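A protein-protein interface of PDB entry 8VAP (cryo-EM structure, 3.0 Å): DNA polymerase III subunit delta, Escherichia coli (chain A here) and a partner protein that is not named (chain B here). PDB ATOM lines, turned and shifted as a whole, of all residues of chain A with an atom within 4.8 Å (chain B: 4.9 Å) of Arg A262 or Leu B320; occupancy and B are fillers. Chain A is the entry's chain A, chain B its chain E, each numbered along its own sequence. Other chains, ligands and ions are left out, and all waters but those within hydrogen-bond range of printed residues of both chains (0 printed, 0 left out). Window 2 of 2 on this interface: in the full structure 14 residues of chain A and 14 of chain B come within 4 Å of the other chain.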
ATOM      1  N   VAL A 258     -10.870  -1.324 -14.812  1.00  0.00           N
ATOM      2  CA  VAL A 258     -10.507  -2.621 -14.248  1.00  0.00           C
ATOM      3  C   VAL A 258      -9.350  -2.469 -13.271  1.00  0.00           C
ATOM      4  O   VAL A 258      -9.348  -3.074 -12.191  1.00  0.00           O
ATOM      5  CB  VAL A 258     -10.179  -3.625 -15.369  1.00  0.00           C
ATOM      6  CG1 VAL A 258      -9.510  -4.861 -14.798  1.00  0.00           C
ATOM      7  CG2 VAL A 258     -11.443  -4.019 -16.106  1.00  0.00           C
ATOM      8  N   ASN A 259      -8.349  -1.661 -13.630  1.00  0.00           N
ATOM      9  CA  ASN A 259      -7.266  -1.386 -12.690  1.00  0.00           C
ATOM     10  C   ASN A 259      -7.802  -0.763 -11.407  1.00  0.00           C
ATOM     11  O   ASN A 259      -7.405  -1.151 -10.299  1.00  0.00           O
ATOM     12  CB  ASN A 259      -6.227  -0.465 -13.330  1.00  0.00           C
ATOM     13  CG  ASN A 259      -5.372  -1.174 -14.355  1.00  0.00           C
ATOM     14  OD1 ASN A 259      -5.327  -2.401 -14.398  1.00  0.00           O
ATOM     15  ND2 ASN A 259      -4.682  -0.403 -15.186  1.00  0.00           N
ATOM     16  N   LEU A 260      -8.716   0.201 -11.541  1.00  0.00           N
ATOM     17  CA  LEU A 260      -9.279   0.862 -10.366  1.00  0.00           C
ATOM     18  C   LEU A 260     -10.040  -0.122  -9.486  1.00  0.00           C
ATOM     19  O   LEU A 260      -9.887  -0.123  -8.259  1.00  0.00           O
ATOM     20  CB  LEU A 260     -10.192   2.005 -10.804  1.00  0.00           C
ATOM     21  CG  LEU A 260      -9.484   3.253 -11.324  1.00  0.00           C
ATOM     22  CD1 LEU A 260     -10.501   4.323 -11.654  1.00  0.00           C
ATOM     23  CD2 LEU A 260      -8.483   3.757 -10.303  1.00  0.00           C
ATOM     24  N   LYS A 261     -10.870  -0.969 -10.097  1.00  0.00           N
ATOM     25  CA  LYS A 261     -11.649  -1.932  -9.324  1.00  0.00           C
ATOM     26  C   LYS A 261     -10.745  -2.948  -8.641  1.00  0.00           C
ATOM     27  O   LYS A 261     -11.018  -3.368  -7.510  1.00  0.00           O
ATOM     28  CB  LYS A 261     -12.662  -2.636 -10.226  1.00  0.00           C
ATOM     29  CG  LYS A 261     -13.588  -3.586  -9.490  1.00  0.00           C
ATOM     30  CD  LYS A 261     -14.457  -2.842  -8.493  1.00  0.00           C
ATOM     31  CE  LYS A 261     -15.504  -3.757  -7.881  1.00  0.00           C
ATOM     32  NZ  LYS A 261     -16.293  -3.070  -6.821  1.00  0.00           N
ATOM     33  N   ARG A 262      -9.670  -3.364  -9.315  1.00  0.00           N
ATOM     34  CA  ARG A 262      -8.725  -4.285  -8.697  1.00  0.00           C
ATOM     35  C   ARG A 262      -8.029  -3.645  -7.504  1.00  0.00           C
ATOM     36  O   ARG A 262      -7.836  -4.293  -6.469  1.00  0.00           O
ATOM     37  CB  ARG A 262      -7.700  -4.753  -9.727  1.00  0.00           C
ATOM     38  CG  ARG A 262      -6.731  -5.794  -9.200  1.00  0.00           C
ATOM     39  CD  ARG A 262      -5.800  -6.268 -10.294  1.00  0.00           C
ATOM     40  NE  ARG A 262      -6.545  -6.913 -11.366  1.00  0.00           N
ATOM     41  CZ  ARG A 262      -6.930  -8.181 -11.349  1.00  0.00           C
ATOM     42  NH1 ARG A 262      -6.642  -8.977 -10.333  1.00  0.00           N
ATOM     43  NH2 ARG A 262      -7.621  -8.663 -12.379  1.00  0.00           N
ATOM     44  N   GLN A 263      -7.650  -2.376  -7.625  1.00  0.00           N
ATOM     45  CA  GLN A 263      -6.931  -1.701  -6.552  1.00  0.00           C
ATOM     46  C   GLN A 263      -7.852  -1.085  -5.505  1.00  0.00           C
ATOM     47  O   GLN A 263      -7.356  -0.503  -4.535  1.00  0.00           O
ATOM     48  CB  GLN A 263      -6.015  -0.621  -7.133  1.00  0.00           C
ATOM     49  CG  GLN A 263      -4.738  -1.164  -7.750  1.00  0.00           C
ATOM     50  CD  GLN A 263      -4.028  -0.141  -8.615  1.00  0.00           C
ATOM     51  OE1 GLN A 263      -4.665   0.665  -9.294  1.00  0.00           O
ATOM     52  NE2 GLN A 263      -2.701  -0.167  -8.594  1.00  0.00           N
ATOM     53  N   SER A 264      -9.173  -1.193  -5.674  1.00  0.00           N
ATOM     54  CA  SER A 264     -10.097  -0.571  -4.729  1.00  0.00           C
ATOM     55  C   SER A 264      -9.971  -1.180  -3.337  1.00  0.00           C
ATOM     56  O   SER A 264     -10.022  -0.461  -2.331  1.00  0.00           O
ATOM     57  CB  SER A 264     -11.533  -0.695  -5.237  1.00  0.00           C
ATOM     58  OG  SER A 264     -12.075  -1.968  -4.928  1.00  0.00           O
ATOM     59  N   ALA A 265      -9.812  -2.502  -3.256  1.00  0.00           N
ATOM     60  CA  ALA A 265      -9.671  -3.164  -1.965  1.00  0.00           C
ATOM     61  C   ALA A 265      -8.353  -2.841  -1.273  1.00  0.00           C
ATOM     62  O   ALA A 265      -8.202  -3.161  -0.090  1.00  0.00           O
ATOM     63  CB  ALA A 265      -9.807  -4.678  -2.133  1.00  0.00           C
ATOM     64  N   GLN A 295     -16.549  -7.437 -10.379  1.00  0.00           N
ATOM     65  CA  GLN A 295     -15.390  -7.988 -11.074  1.00  0.00           C
ATOM     66  C   GLN A 295     -15.816  -8.968 -12.161  1.00  0.00           C
ATOM     67  O   GLN A 295     -15.203  -9.022 -13.234  1.00  0.00           O
ATOM     68  CB  GLN A 295     -14.452  -8.661 -10.073  1.00  0.00           C
ATOM     69  CG  GLN A 295     -13.172  -9.204 -10.685  1.00  0.00           C
ATOM     70  CD  GLN A 295     -12.321  -8.120 -11.313  1.00  0.00           C
ATOM     71  OE1 GLN A 295     -12.270  -7.985 -12.534  1.00  0.00           O
ATOM     72  NE2 GLN A 295     -11.644  -7.341 -10.477  1.00  0.00           N
ATOM     73  N   LEU A 298     -16.901  -6.977 -15.101  1.00  0.00           N
ATOM     74  CA  LEU A 298     -15.736  -6.442 -15.797  1.00  0.00           C
ATOM     75  C   LEU A 298     -15.061  -7.507 -16.650  1.00  0.00           C
ATOM     76  O   LEU A 298     -14.655  -7.237 -17.787  1.00  0.00           O
ATOM     77  CB  LEU A 298     -14.747  -5.857 -14.791  1.00  0.00           C
ATOM     78  CG  LEU A 298     -15.100  -4.469 -14.264  1.00  0.00           C
ATOM     79  CD1 LEU A 298     -13.964  -3.906 -13.429  1.00  0.00           C
ATOM     80  CD2 LEU A 298     -15.438  -3.541 -15.416  1.00  0.00           C
ATOM     81  N   ARG A 299     -14.922  -8.724 -16.118  1.00  0.00           N
ATOM     82  CA  ARG A 299     -14.316  -9.799 -16.896  1.00  0.00           C
ATOM     83  C   ARG A 299     -15.159 -10.136 -18.119  1.00  0.00           C
ATOM     84  O   ARG A 299     -14.624 -10.353 -19.213  1.00  0.00           O
ATOM     85  CB  ARG A 299     -14.116 -11.038 -16.025  1.00  0.00           C
ATOM     86  CG  ARG A 299     -13.360 -12.158 -16.718  1.00  0.00           C
ATOM     87  CD  ARG A 299     -13.127 -13.334 -15.786  1.00  0.00           C
ATOM     88  NE  ARG A 299     -14.376 -13.976 -15.395  1.00  0.00           N
ATOM     89  CZ  ARG A 299     -14.852 -13.994 -14.158  1.00  0.00           C
ATOM     90  NH1 ARG A 299     -14.208 -13.411 -13.161  1.00  0.00           N
ATOM     91  NH2 ARG A 299     -16.004 -14.613 -13.916  1.00  0.00           N
ATOM     92  N   VAL A 302     -14.649  -7.402 -20.694  1.00  0.00           N
ATOM     93  CA  VAL A 302     -13.369  -7.557 -21.379  1.00  0.00           C
ATOM     94  C   VAL A 302     -13.444  -8.691 -22.391  1.00  0.00           C
ATOM     95  O   VAL A 302     -12.931  -8.577 -23.510  1.00  0.00           O
ATOM     96  CB  VAL A 302     -12.234  -7.774 -20.360  1.00  0.00           C
ATOM     97  CG1 VAL A 302     -10.945  -8.143 -21.073  1.00  0.00           C
ATOM     98  CG2 VAL A 302     -12.030  -6.527 -19.527  1.00  0.00           C
ATOM     99  N   ASP B 231      -2.620 -13.678  -8.681  1.00  0.00           N
ATOM    100  CA  ASP B 231      -2.558 -12.292  -9.138  1.00  0.00           C
ATOM    101  C   ASP B 231      -1.884 -12.212 -10.504  1.00  0.00           C
ATOM    102  O   ASP B 231      -0.963 -11.426 -10.730  1.00  0.00           O
ATOM    103  CB  ASP B 231      -1.829 -11.420  -8.121  1.00  0.00           C
ATOM    104  CG  ASP B 231      -2.201  -9.958  -8.238  1.00  0.00           C
ATOM    105  OD1 ASP B 231      -3.035  -9.623  -9.104  1.00  0.00           O
ATOM    106  OD2 ASP B 231      -1.657  -9.142  -7.464  1.00  0.00           O
ATOM    107  N   TYR B 233      -2.920 -10.993 -13.207  1.00  0.00           N
ATOM    108  CA  TYR B 233      -3.102  -9.731 -13.914  1.00  0.00           C
ATOM    109  C   TYR B 233      -1.863  -8.853 -13.812  1.00  0.00           C
ATOM    110  O   TYR B 233      -1.550  -8.106 -14.749  1.00  0.00           O
ATOM    111  CB  TYR B 233      -4.323  -8.994 -13.370  1.00  0.00           C
ATOM    112  CG  TYR B 233      -4.607  -7.684 -14.068  1.00  0.00           C
ATOM    113  CD1 TYR B 233      -5.428  -7.635 -15.184  1.00  0.00           C
ATOM    114  CD2 TYR B 233      -4.057  -6.496 -13.608  1.00  0.00           C
ATOM    115  CE1 TYR B 233      -5.690  -6.442 -15.824  1.00  0.00           C
ATOM    116  CE2 TYR B 233      -4.310  -5.300 -14.242  1.00  0.00           C
ATOM    117  CZ  TYR B 233      -5.129  -5.278 -15.350  1.00  0.00           C
ATOM    118  OH  TYR B 233      -5.386  -4.084 -15.983  1.00  0.00           O
ATOM    119  N   THR B 316      -4.594  -8.625 -21.477  1.00  0.00           N
ATOM    120  CA  THR B 316      -5.446  -8.418 -20.310  1.00  0.00           C
ATOM    121  C   THR B 316      -6.556  -9.459 -20.245  1.00  0.00           C
ATOM    122  O   THR B 316      -6.853  -9.997 -19.170  1.00  0.00           O
ATOM    123  CB  THR B 316      -6.037  -7.009 -20.341  1.00  0.00           C
ATOM    124  OG1 THR B 316      -4.977  -6.046 -20.325  1.00  0.00           O
ATOM    125  CG2 THR B 316      -6.935  -6.783 -19.140  1.00  0.00           C
ATOM    126  N   ASP B 317      -7.177  -9.760 -21.387  1.00  0.00           N
ATOM    127  CA  ASP B 317      -8.210 -10.790 -21.420  1.00  0.00           C
ATOM    128  C   ASP B 317      -7.637 -12.157 -21.076  1.00  0.00           C
ATOM    129  O   ASP B 317      -8.273 -12.945 -20.368  1.00  0.00           O
ATOM    130  CB  ASP B 317      -8.867 -10.823 -22.795  1.00  0.00           C
ATOM    131  CG  ASP B 317     -10.235 -11.448 -22.762  1.00  0.00           C
ATOM    132  OD1 ASP B 317     -10.341 -12.647 -22.435  1.00  0.00           O
ATOM    133  OD2 ASP B 317     -11.206 -10.733 -23.057  1.00  0.00           O
ATOM    134  N   LEU B 318      -6.442 -12.460 -21.587  1.00  0.00           N
ATOM    135  CA  LEU B 318      -5.765 -13.705 -21.242  1.00  0.00           C
ATOM    136  C   LEU B 318      -5.561 -13.823 -19.738  1.00  0.00           C
ATOM    137  O   LEU B 318      -5.846 -14.869 -19.141  1.00  0.00           O
ATOM    138  CB  LEU B 318      -4.425 -13.772 -21.974  1.00  0.00           C
ATOM    139  CG  LEU B 318      -3.470 -14.934 -21.717  1.00  0.00           C
ATOM    140  CD1 LEU B 318      -4.118 -16.254 -22.056  1.00  0.00           C
ATOM    141  CD2 LEU B 318      -2.194 -14.739 -22.518  1.00  0.00           C
ATOM    142  N   LEU B 319      -5.075 -12.753 -19.111  1.00  0.00           N
ATOM    143  CA  LEU B 319      -4.823 -12.790 -17.676  1.00  0.00           C
ATOM    144  C   LEU B 319      -6.119 -12.923 -16.885  1.00  0.00           C
ATOM    145  O   LEU B 319      -6.174 -13.661 -15.893  1.00  0.00           O
ATOM    146  CB  LEU B 319      -4.054 -11.540 -17.256  1.00  0.00           C
ATOM    147  CG  LEU B 319      -2.655 -11.458 -17.866  1.00  0.00           C
ATOM    148  CD1 LEU B 319      -1.930 -10.219 -17.383  1.00  0.00           C
ATOM    149  CD2 LEU B 319      -1.859 -12.710 -17.547  1.00  0.00           C
ATOM    150  N   LEU B 320      -7.175 -12.223 -17.306  1.00  0.00           N
ATOM    151  CA  LEU B 320      -8.456 -12.347 -16.618  1.00  0.00           C
ATOM    152  C   LEU B 320      -9.021 -13.754 -16.755  1.00  0.00           C
ATOM    153  O   LEU B 320      -9.604 -14.293 -15.806  1.00  0.00           O
ATOM    154  CB  LEU B 320      -9.447 -11.314 -17.151  1.00  0.00           C
ATOM    155  CG  LEU B 320      -9.175  -9.851 -16.795  1.00  0.00           C
ATOM    156  CD1 LEU B 320     -10.414  -9.003 -17.038  1.00  0.00           C
ATOM    157  CD2 LEU B 320      -8.700  -9.718 -15.358  1.00  0.00           C
ATOM    158  N   ARG B 321      -8.866 -14.367 -17.930  1.00  0.00           N
ATOM    159  CA  ARG B 321      -9.324 -15.740 -18.114  1.00  0.00           C
ATOM    160  C   ARG B 321      -8.530 -16.708 -17.247  1.00  0.00           C
ATOM    161  O   ARG B 321      -9.096 -17.659 -16.698  1.00  0.00           O
ATOM    162  CB  ARG B 321      -9.228 -16.132 -19.585  1.00  0.00           C
ATOM    163  CG  ARG B 321     -10.547 -16.053 -20.328  1.00  0.00           C
ATOM    164  CD  ARG B 321     -10.619 -17.110 -21.412  1.00  0.00           C
ATOM    165  NE  ARG B 321      -9.493 -17.014 -22.330  1.00  0.00           N
ATOM    166  CZ  ARG B 321      -9.385 -16.109 -23.293  1.00  0.00           C
ATOM    167  NH1 ARG B 321     -10.328 -15.206 -23.501  1.00  0.00           N
ATOM    168  NH2 ARG B 321      -8.303 -16.110 -24.065  1.00  0.00           N
ATOM    169  N   ILE B 322      -7.220 -16.491 -17.118  1.00  0.00           N
ATOM    170  CA  ILE B 322      -6.422 -17.318 -16.214  1.00  0.00           C
ATOM    171  C   ILE B 322      -6.919 -17.168 -14.782  1.00  0.00           C
ATOM    172  O   ILE B 322      -7.071 -18.156 -14.050  1.00  0.00           O
ATOM    173  CB  ILE B 322      -4.929 -16.963 -16.336  1.00  0.00           C
ATOM    174  CG1 ILE B 322      -4.400 -17.341 -17.718  1.00  0.00           C
ATOM    175  CG2 ILE B 322      -4.127 -17.655 -15.250  1.00  0.00           C
ATOM    176  CD1 ILE B 322      -2.938 -17.018 -17.913  1.00  0.00           C
ATOM    177  N   GLU B 323      -7.188 -15.929 -14.364  1.00  0.00           N
ATOM    178  CA  GLU B 323      -7.718 -15.690 -13.025  1.00  0.00           C
ATOM    179  C   GLU B 323      -9.038 -16.421 -12.816  1.00  0.00           C
ATOM    180  O   GLU B 323      -9.268 -17.011 -11.754  1.00  0.00           O
ATOM    181  CB  GLU B 323      -7.901 -14.190 -12.794  1.00  0.00           C
ATOM    182  CG  GLU B 323      -6.606 -13.415 -12.640  1.00  0.00           C
ATOM    183  CD  GLU B 323      -5.862 -13.789 -11.380  1.00  0.00           C
ATOM    184  OE1 GLU B 323      -6.520 -14.209 -10.406  1.00  0.00           O
ATOM    185  OE2 GLU B 323      -4.621 -13.662 -11.359  1.00  0.00           O
ATOM    186  N   HIS B 324      -9.919 -16.386 -13.815  1.00  0.00           N
ATOM    187  CA  HIS B 324     -11.184 -17.105 -13.712  1.00  0.00           C
ATOM    188  C   HIS B 324     -10.957 -18.610 -13.628  1.00  0.00           C
ATOM    189  O   HIS B 324     -11.662 -19.313 -12.895  1.00  0.00           O
ATOM    190  CB  HIS B 324     -12.081 -16.768 -14.900  1.00  0.00           C
ATOM    191  CG  HIS B 324     -13.387 -17.496 -14.897  1.00  0.00           C
ATOM    192  ND1 HIS B 324     -14.278 -17.419 -13.849  1.00  0.00           N
ATOM    193  CD2 HIS B 324     -13.954 -18.316 -15.812  1.00  0.00           C
ATOM    194  CE1 HIS B 324     -15.338 -18.159 -14.119  1.00  0.00           C
ATOM    195  NE2 HIS B 324     -15.167 -18.714 -15.305  1.00  0.00           N
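Of chain B, only Asp B231, Tyr B233 and Leu B320 come within 4 Å of Arg A262. Of the printed residues of chain B, Arg A299 touches Leu B320 (3.7 Å) and His B324 (3.3 Å). Printed residues of chain B within 4 Å of Val A302: Asp B317 and Leu B320. Of the printed residues of chain A, Asp B231 touches Arg A262 (3.9 Å). Leu B320 touches three residues of chain A. The nearest residue of chain A that does not touch Leu B320 is Leu A298 (4.7 Å).
NH1 of Arg A262 is in salt-bridge range of OD1 of Asp B231 (3.9 Å). A ring nitrogen (ND1) of His B324 sits at hydrogen-bond distance from the guanidinium group (NH2) of Arg A299. The side-chain amide oxygen (OD1) of Asn A259 sits close to the side-chain hydroxyl (OH) of Tyr B233 (2.3 Å). The side-chain carboxylate (OD2) of Asp B317 lies close to the backbone carbonyl oxygen (O) of Val A302.
CD2 of Tyr B233 touches NE of Arg A262, at 3.4 Å. Arg A262 touches Leu B320. Leu B320 touches Arg A299. CD1 of Leu B320 touches CG2 of Val A302 (3.9 Å).
Hydrophobic or aromatic side chains of chain B within 4 Å of the printed part of chain A: Tyr B233, Leu B320 and His B324. Among the printed residues, 8 pairs touch across the chains.
OE1 of Gln A263 sits close to O of Asn A259, at 3.4 Å. The backbone NH of Asp B231 sits close to the side-chain carboxylate of Glu B323, at 3.3 Å. OD1 of Asp B317 is in salt-bridge range of NH1 of Arg B321 (2.8 Å).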
